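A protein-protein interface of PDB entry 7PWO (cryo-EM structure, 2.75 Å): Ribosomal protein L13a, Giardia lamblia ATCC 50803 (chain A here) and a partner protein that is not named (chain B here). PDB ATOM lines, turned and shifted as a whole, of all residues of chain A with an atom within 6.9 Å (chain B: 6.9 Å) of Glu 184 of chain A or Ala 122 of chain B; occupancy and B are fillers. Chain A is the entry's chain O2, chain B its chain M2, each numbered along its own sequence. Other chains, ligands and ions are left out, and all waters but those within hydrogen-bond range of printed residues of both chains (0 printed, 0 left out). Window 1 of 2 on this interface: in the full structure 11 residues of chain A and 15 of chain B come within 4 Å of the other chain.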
ATOM      1  N   ALA A 178     -13.919  22.852  -0.417  1.00  0.00           N
ATOM      2  CA  ALA A 178     -13.356  21.660  -1.018  1.00  0.00           C
ATOM      3  C   ALA A 178     -14.235  20.460  -0.688  1.00  0.00           C
ATOM      4  O   ALA A 178     -13.760  19.443  -0.178  1.00  0.00           O
ATOM      5  CB  ALA A 178     -11.930  21.437  -0.536  1.00  0.00           C
ATOM      6  N   ALA A 179     -15.528  20.594  -0.987  1.00  0.00           N
ATOM      7  CA  ALA A 179     -16.447  19.480  -1.152  1.00  0.00           C
ATOM      8  C   ALA A 179     -16.535  19.051  -2.601  1.00  0.00           C
ATOM      9  O   ALA A 179     -17.568  18.529  -3.040  1.00  0.00           O
ATOM     10  CB  ALA A 179     -17.827  19.848  -0.612  1.00  0.00           C
ATOM     11  N   GLU A 180     -15.468  19.296  -3.367  1.00  0.00           N
ATOM     12  CA  GLU A 180     -15.452  19.055  -4.802  1.00  0.00           C
ATOM     13  C   GLU A 180     -14.235  18.241  -5.235  1.00  0.00           C
ATOM     14  O   GLU A 180     -13.869  18.271  -6.412  1.00  0.00           O
ATOM     15  CB  GLU A 180     -15.504  20.384  -5.560  1.00  0.00           C
ATOM     16  CG  GLU A 180     -16.811  21.137  -5.372  1.00  0.00           C
ATOM     17  CD  GLU A 180     -17.995  20.407  -5.995  1.00  0.00           C
ATOM     18  OE1 GLU A 180     -17.800  19.721  -7.016  1.00  0.00           O
ATOM     19  OE2 GLU A 180     -19.116  20.511  -5.455  1.00  0.00           O
ATOM     20  N   LYS A 181     -13.591  17.526  -4.315  1.00  0.00           N
ATOM     21  CA  LYS A 181     -12.491  16.630  -4.663  1.00  0.00           C
ATOM     22  C   LYS A 181     -13.000  15.201  -4.471  1.00  0.00           C
ATOM     23  O   LYS A 181     -13.034  14.671  -3.350  1.00  0.00           O
ATOM     24  CB  LYS A 181     -11.248  16.942  -3.836  1.00  0.00           C
ATOM     25  CG  LYS A 181      -9.935  16.829  -4.614  1.00  0.00           C
ATOM     26  CD  LYS A 181      -8.727  16.910  -3.685  1.00  0.00           C
ATOM     27  CE  LYS A 181      -7.436  16.407  -4.324  1.00  0.00           C
ATOM     28  NZ  LYS A 181      -6.434  15.984  -3.296  1.00  0.00           N
ATOM     29  N   ASP A 182     -13.436  14.588  -5.575  1.00  0.00           N
ATOM     30  CA  ASP A 182     -13.972  13.241  -5.473  1.00  0.00           C
ATOM     31  C   ASP A 182     -12.895  12.242  -5.088  1.00  0.00           C
ATOM     32  O   ASP A 182     -13.213  11.213  -4.497  1.00  0.00           O
ATOM     33  CB  ASP A 182     -14.646  12.816  -6.781  1.00  0.00           C
ATOM     34  CG  ASP A 182     -15.691  11.727  -6.574  1.00  0.00           C
ATOM     35  OD1 ASP A 182     -15.561  10.938  -5.611  1.00  0.00           O
ATOM     36  OD2 ASP A 182     -16.647  11.654  -7.379  1.00  0.00           O
ATOM     37  N   ALA A 183     -11.626  12.532  -5.370  1.00  0.00           N
ATOM     38  CA  ALA A 183     -10.568  11.694  -4.826  1.00  0.00           C
ATOM     39  C   ALA A 183     -10.524  11.744  -3.303  1.00  0.00           C
ATOM     40  O   ALA A 183      -9.767  10.980  -2.693  1.00  0.00           O
ATOM     41  CB  ALA A 183      -9.220  12.108  -5.411  1.00  0.00           C
ATOM     42  N   GLU A 184     -11.305  12.627  -2.682  1.00  0.00           N
ATOM     43  CA  GLU A 184     -11.534  12.631  -1.244  1.00  0.00           C
ATOM     44  C   GLU A 184     -12.891  12.061  -0.858  1.00  0.00           C
ATOM     45  O   GLU A 184     -13.010  11.426   0.190  1.00  0.00           O
ATOM     46  CB  GLU A 184     -11.418  14.051  -0.690  1.00  0.00           C
ATOM     47  CG  GLU A 184     -10.842  14.122   0.694  1.00  0.00           C
ATOM     48  CD  GLU A 184     -10.785  15.533   1.200  1.00  0.00           C
ATOM     49  OE1 GLU A 184     -11.857  16.120   1.438  1.00  0.00           O
ATOM     50  OE2 GLU A 184      -9.666  16.059   1.338  1.00  0.00           O
ATOM     51  N   LEU A 185     -13.931  12.291  -1.662  1.00  0.00           N
ATOM     52  CA  LEU A 185     -15.221  11.682  -1.327  1.00  0.00           C
ATOM     53  C   LEU A 185     -15.164  10.161  -1.442  1.00  0.00           C
ATOM     54  O   LEU A 185     -15.771   9.439  -0.632  1.00  0.00           O
ATOM     55  CB  LEU A 185     -16.334  12.255  -2.206  1.00  0.00           C
ATOM     56  CG  LEU A 185     -16.878  13.646  -1.851  1.00  0.00           C
ATOM     57  CD1 LEU A 185     -15.897  14.743  -2.165  1.00  0.00           C
ATOM     58  CD2 LEU A 185     -18.177  13.919  -2.581  1.00  0.00           C
ATOM     59  N   GLN A 186     -14.410   9.658  -2.423  1.00  0.00           N
ATOM     60  CA  GLN A 186     -14.303   8.230  -2.681  1.00  0.00           C
ATOM     61  C   GLN A 186     -13.680   7.482  -1.522  1.00  0.00           C
ATOM     62  O   GLN A 186     -13.693   6.246  -1.515  1.00  0.00           O
ATOM     63  CB  GLN A 186     -13.489   7.990  -3.948  1.00  0.00           C
ATOM     64  CG  GLN A 186     -12.029   8.402  -3.860  1.00  0.00           C
ATOM     65  CD  GLN A 186     -11.125   7.269  -3.434  1.00  0.00           C
ATOM     66  OE1 GLN A 186     -11.244   6.146  -3.925  1.00  0.00           O
ATOM     67  NE2 GLN A 186     -10.203   7.559  -2.521  1.00  0.00           N
ATOM     68  N   ARG A 187     -13.119   8.201  -0.565  1.00  0.00           N
ATOM     69  CA  ARG A 187     -12.628   7.629   0.670  1.00  0.00           C
ATOM     70  C   ARG A 187     -13.313   8.151   1.928  1.00  0.00           C
ATOM     71  O   ARG A 187     -13.205   7.500   2.970  1.00  0.00           O
ATOM     72  CB  ARG A 187     -11.128   7.871   0.787  1.00  0.00           C
ATOM     73  CG  ARG A 187     -10.871   9.309   0.886  1.00  0.00           C
ATOM     74  CD  ARG A 187      -9.445   9.580   0.993  1.00  0.00           C
ATOM     75  NE  ARG A 187      -9.134   8.988   2.277  1.00  0.00           N
ATOM     76  CZ  ARG A 187      -9.323   9.615   3.427  1.00  0.00           C
ATOM     77  NH1 ARG A 187      -9.895  10.807   3.434  1.00  0.00           N
ATOM     78  NH2 ARG A 187      -9.031   9.017   4.565  1.00  0.00           N
ATOM     79  N   ILE A 188     -13.997   9.297   1.880  1.00  0.00           N
ATOM     80  CA  ILE A 188     -14.848   9.667   3.014  1.00  0.00           C
ATOM     81  C   ILE A 188     -15.974   8.659   3.163  1.00  0.00           C
ATOM     82  O   ILE A 188     -16.380   8.325   4.283  1.00  0.00           O
ATOM     83  CB  ILE A 188     -15.383  11.103   2.869  1.00  0.00           C
ATOM     84  CG1 ILE A 188     -14.257  12.114   3.056  1.00  0.00           C
ATOM     85  CG2 ILE A 188     -16.477  11.388   3.889  1.00  0.00           C
ATOM     86  CD1 ILE A 188     -13.483  11.921   4.327  1.00  0.00           C
ATOM     87  N   ASN A 189     -16.468   8.123   2.046  1.00  0.00           N
ATOM     88  CA  ASN A 189     -17.424   7.022   2.139  1.00  0.00           C
ATOM     89  C   ASN A 189     -16.813   5.807   2.844  1.00  0.00           C
ATOM     90  O   ASN A 189     -17.491   5.118   3.621  1.00  0.00           O
ATOM     91  CB  ASN A 189     -17.916   6.640   0.750  1.00  0.00           C
ATOM     92  CG  ASN A 189     -18.875   5.462   0.772  1.00  0.00           C
ATOM     93  OD1 ASN A 189     -19.695   5.321   1.683  1.00  0.00           O
ATOM     94  ND2 ASN A 189     -18.756   4.596  -0.221  1.00  0.00           N
ATOM     95  N   ALA A 190     -15.542   5.510   2.569  1.00  0.00           N
ATOM     96  CA  ALA A 190     -14.895   4.383   3.233  1.00  0.00           C
ATOM     97  C   ALA A 190     -14.703   4.652   4.718  1.00  0.00           C
ATOM     98  O   ALA A 190     -14.869   3.752   5.549  1.00  0.00           O
ATOM     99  CB  ALA A 190     -13.554   4.079   2.575  1.00  0.00           C
ATOM    100  N   GLU A 191     -14.322   5.882   5.064  1.00  0.00           N
ATOM    101  CA  GLU A 191     -14.306   6.276   6.462  1.00  0.00           C
ATOM    102  C   GLU A 191     -15.651   5.991   7.104  1.00  0.00           C
ATOM    103  O   GLU A 191     -15.720   5.440   8.212  1.00  0.00           O
ATOM    104  CB  GLU A 191     -13.995   7.760   6.603  1.00  0.00           C
ATOM    105  CG  GLU A 191     -12.620   8.193   6.162  1.00  0.00           C
ATOM    106  CD  GLU A 191     -11.524   7.633   7.013  1.00  0.00           C
ATOM    107  OE1 GLU A 191     -11.731   7.413   8.218  1.00  0.00           O
ATOM    108  OE2 GLU A 191     -10.423   7.468   6.465  1.00  0.00           O
ATOM    109  N   ARG B 117      -4.511   8.399   7.206  1.00  0.00           N
ATOM    110  CA  ARG B 117      -3.337   8.985   6.571  1.00  0.00           C
ATOM    111  C   ARG B 117      -3.716   9.753   5.313  1.00  0.00           C
ATOM    112  O   ARG B 117      -3.399  10.945   5.180  1.00  0.00           O
ATOM    113  CB  ARG B 117      -2.300   7.912   6.245  1.00  0.00           C
ATOM    114  CG  ARG B 117      -1.072   8.495   5.603  1.00  0.00           C
ATOM    115  CD  ARG B 117      -0.344   9.376   6.562  1.00  0.00           C
ATOM    116  NE  ARG B 117       0.875   9.933   5.987  1.00  0.00           N
ATOM    117  CZ  ARG B 117       1.597  10.869   6.588  1.00  0.00           C
ATOM    118  NH1 ARG B 117       1.217  11.318   7.771  1.00  0.00           N
ATOM    119  NH2 ARG B 117       2.686  11.353   6.015  1.00  0.00           N
ATOM    120  N   GLU B 118      -4.411   9.102   4.378  1.00  0.00           N
ATOM    121  CA  GLU B 118      -4.697   9.908   3.188  1.00  0.00           C
ATOM    122  C   GLU B 118      -5.789  10.961   3.402  1.00  0.00           C
ATOM    123  O   GLU B 118      -5.859  11.901   2.608  1.00  0.00           O
ATOM    124  CB  GLU B 118      -4.963   9.100   1.902  1.00  0.00           C
ATOM    125  CG  GLU B 118      -6.189   8.255   1.765  1.00  0.00           C
ATOM    126  CD  GLU B 118      -5.968   6.906   2.330  1.00  0.00           C
ATOM    127  OE1 GLU B 118      -4.987   6.758   3.060  1.00  0.00           O
ATOM    128  OE2 GLU B 118      -6.748   5.987   2.021  1.00  0.00           O
ATOM    129  N   ARG B 119      -6.583  10.909   4.477  1.00  0.00           N
ATOM    130  CA  ARG B 119      -7.381  12.101   4.789  1.00  0.00           C
ATOM    131  C   ARG B 119      -6.489  13.285   5.127  1.00  0.00           C
ATOM    132  O   ARG B 119      -6.708  14.403   4.638  1.00  0.00           O
ATOM    133  CB  ARG B 119      -8.364  11.870   5.937  1.00  0.00           C
ATOM    134  CG  ARG B 119      -9.194  13.131   6.174  1.00  0.00           C
ATOM    135  CD  ARG B 119     -10.269  13.041   7.243  1.00  0.00           C
ATOM    136  NE  ARG B 119     -11.379  12.167   6.905  1.00  0.00           N
ATOM    137  CZ  ARG B 119     -12.326  11.825   7.766  1.00  0.00           C
ATOM    138  NH1 ARG B 119     -13.319  11.037   7.392  1.00  0.00           N
ATOM    139  NH2 ARG B 119     -12.273  12.262   9.013  1.00  0.00           N
ATOM    140  N   LYS B 120      -5.494  13.061   5.984  1.00  0.00           N
ATOM    141  CA  LYS B 120      -4.569  14.136   6.328  1.00  0.00           C
ATOM    142  C   LYS B 120      -3.895  14.685   5.073  1.00  0.00           C
ATOM    143  O   LYS B 120      -3.795  15.906   4.883  1.00  0.00           O
ATOM    144  CB  LYS B 120      -3.538  13.609   7.325  1.00  0.00           C
ATOM    145  CG  LYS B 120      -2.457  14.577   7.722  1.00  0.00           C
ATOM    146  CD  LYS B 120      -1.361  13.864   8.494  1.00  0.00           C
ATOM    147  CE  LYS B 120      -1.380  14.189   9.971  1.00  0.00           C
ATOM    148  NZ  LYS B 120      -0.133  13.735  10.648  1.00  0.00           N
ATOM    149  N   MET B 121      -3.489  13.791   4.171  1.00  0.00           N
ATOM    150  CA  MET B 121      -2.735  14.227   3.000  1.00  0.00           C
ATOM    151  C   MET B 121      -3.611  14.931   1.968  1.00  0.00           C
ATOM    152  O   MET B 121      -3.158  15.877   1.318  1.00  0.00           O
ATOM    153  CB  MET B 121      -2.017  13.034   2.374  1.00  0.00           C
ATOM    154  CG  MET B 121      -1.129  12.274   3.350  1.00  0.00           C
ATOM    155  SD  MET B 121       0.079  13.195   4.339  1.00  0.00           S
ATOM    156  CE  MET B 121       0.584  14.511   3.241  1.00  0.00           C
ATOM    157  N   ALA B 122      -4.855  14.488   1.787  1.00  0.00           N
ATOM    158  CA  ALA B 122      -5.749  15.188   0.875  1.00  0.00           C
ATOM    159  C   ALA B 122      -6.115  16.567   1.407  1.00  0.00           C
ATOM    160  O   ALA B 122      -6.119  17.549   0.651  1.00  0.00           O
ATOM    161  CB  ALA B 122      -7.002  14.355   0.634  1.00  0.00           C
ATOM    162  N   MET B 123      -6.434  16.662   2.701  1.00  0.00           N
ATOM    163  CA  MET B 123      -6.691  17.976   3.274  1.00  0.00           C
ATOM    164  C   MET B 123      -5.487  18.892   3.151  1.00  0.00           C
ATOM    165  O   MET B 123      -5.656  20.102   2.986  1.00  0.00           O
ATOM    166  CB  MET B 123      -7.130  17.853   4.731  1.00  0.00           C
ATOM    167  CG  MET B 123      -8.565  17.397   4.913  1.00  0.00           C
ATOM    168  SD  MET B 123      -9.659  17.979   3.601  1.00  0.00           S
ATOM    169  CE  MET B 123      -9.729  19.744   3.922  1.00  0.00           C
ATOM    170  N   LYS B 124      -4.267  18.345   3.174  1.00  0.00           N
ATOM    171  CA  LYS B 124      -3.125  19.233   2.966  1.00  0.00           C
ATOM    172  C   LYS B 124      -2.978  19.647   1.498  1.00  0.00           C
ATOM    173  O   LYS B 124      -2.754  20.830   1.203  1.00  0.00           O
ATOM    174  CB  LYS B 124      -1.847  18.577   3.476  1.00  0.00           C
ATOM    175  CG  LYS B 124      -0.639  19.489   3.439  1.00  0.00           C
ATOM    176  CD  LYS B 124       0.573  18.767   3.965  1.00  0.00           C
ATOM    177  CE  LYS B 124       0.458  18.553   5.467  1.00  0.00           C
ATOM    178  NZ  LYS B 124       0.507  19.808   6.254  1.00  0.00           N
ATOM    179  N   ARG B 125      -3.133  18.697   0.567  1.00  0.00           N
ATOM    180  CA  ARG B 125      -3.072  18.987  -0.865  1.00  0.00           C
ATOM    181  C   ARG B 125      -4.200  19.886  -1.338  1.00  0.00           C
ATOM    182  O   ARG B 125      -4.145  20.363  -2.474  1.00  0.00           O
ATOM    183  CB  ARG B 125      -3.097  17.699  -1.695  1.00  0.00           C
ATOM    184  CG  ARG B 125      -1.722  17.127  -1.994  1.00  0.00           C
ATOM    185  CD  ARG B 125      -1.741  15.632  -2.206  1.00  0.00           C
ATOM    186  NE  ARG B 125      -0.412  15.065  -2.032  1.00  0.00           N
ATOM    187  CZ  ARG B 125      -0.145  14.011  -1.274  1.00  0.00           C
ATOM    188  NH1 ARG B 125      -1.123  13.408  -0.624  1.00  0.00           N
ATOM    189  NH2 ARG B 125       1.097  13.562  -1.166  1.00  0.00           N
ATOM    190  N   ILE B 126      -5.228  20.094  -0.522  1.00  0.00           N
ATOM    191  CA  ILE B 126      -6.196  21.147  -0.808  1.00  0.00           C
ATOM    192  C   ILE B 126      -5.793  22.444  -0.114  1.00  0.00           C
ATOM    193  O   ILE B 126      -5.648  23.477  -0.773  1.00  0.00           O
ATOM    194  CB  ILE B 126      -7.623  20.759  -0.399  1.00  0.00           C
ATOM    195  CG1 ILE B 126      -8.122  19.558  -1.202  1.00  0.00           C
ATOM    196  CG2 ILE B 126      -8.528  21.948  -0.571  1.00  0.00           C
ATOM    197  CD1 ILE B 126      -9.408  18.974  -0.672  1.00  0.00           C
ATOM    198  N   ALA B 127      -5.615  22.413   1.217  1.00  0.00           N
ATOM    199  CA  ALA B 127      -5.408  23.650   1.966  1.00  0.00           C
ATOM    200  C   ALA B 127      -4.190  24.426   1.495  1.00  0.00           C
ATOM    201  O   ALA B 127      -4.134  25.642   1.704  1.00  0.00           O
ATOM    202  CB  ALA B 127      -5.284  23.364   3.463  1.00  0.00           C
ATOM    203  N   MET B 128      -3.221  23.768   0.857  1.00  0.00           N
ATOM    204  CA  MET B 128      -2.193  24.513   0.142  1.00  0.00           C
ATOM    205  C   MET B 128      -2.730  24.936  -1.219  1.00  0.00           C
ATOM    206  O   MET B 128      -2.092  24.689  -2.248  1.00  0.00           O
ATOM    207  CB  MET B 128      -0.918  23.679  -0.030  1.00  0.00           C
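The side-chain carboxylate (OE2) of Glu 118 of chain B lies within salt-bridge range of the guanidinium group (NE) of Arg 187 of chain A (3.8 Å). The side-chain carboxylate (OE2) of Glu 184 of chain A sits close to the side-chain sulfur (SD) of Met 123 of chain B. The guanidinium group (NH2) of Arg 187 of chain A lies close to the backbone NH (N) of Arg 119 of chain B.
NH2 of Arg 187 of chain A is in salt-bridge range of OE2 of Glu 191 of chain A, 2.8 Å away.
CB of Ala 178 of chain A touches CG2 of Ile 126 of chain B, 3.4 Å away. Ile 126 of chain B touches Lys 181 of chain A (CG1 to CD, 3.7 Å). Glu 184 of chain A touches Ala 122 of chain B. Ile 126 of chain B touches Glu 184 of chain A. Ile 188 of chain A touches Arg 119 of chain B (CD1 to NH1, 3.2 Å). Glu 191 of chain A touches Arg 119 of chain B (CG to NH1, 3.2 Å).
Of chain B, only Ala 122 (3.2 Å), Met 123 (3.0 Å) and Ile 126 (3.6 Å) come within 4 Å of Glu 184 of chain A. Of the printed residues of chain B, Lys 181 of chain A touches Ile 126 (3.7 Å). Of the printed residues of chain A, Met 123 of chain B touches Glu 184 (3.0 Å). The nearest residue of chain B that does not touch Glu 184 of chain A is Arg 119 of chain B (4.7 Å). The nearest residue of chain A that does not touch Ala 122 of chain B is Lys 181 of chain A (4.3 Å). The nearest printed residue of chain B that does not touch Glu 191 of chain A is Glu 118 of chain B (6.0 Å).
Of the 14 printed residues of chain A, 6 touch a printed residue of chain B. Printed residues of chain A that touch a printed residue of chain B: Ala 178, Lys 181, Glu 184, Arg 187, Ile 188 and Glu 191. Printed residues of chain B that touch a printed residue of chain A: Glu 118, Arg 119, Ala 122, Met 123 and Ile 126. Hydrophobic or aromatic side chains of chain B that line the printed part of chain A: Ala 122, Met 123 and Ile 126. Among the printed residues, Asp or Glu carboxylates within 4 Å of a Lys or Arg side-chain nitrogen of the other chain: Arg 187 of chain A with Glu 118 of chain B (3.8 Å).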
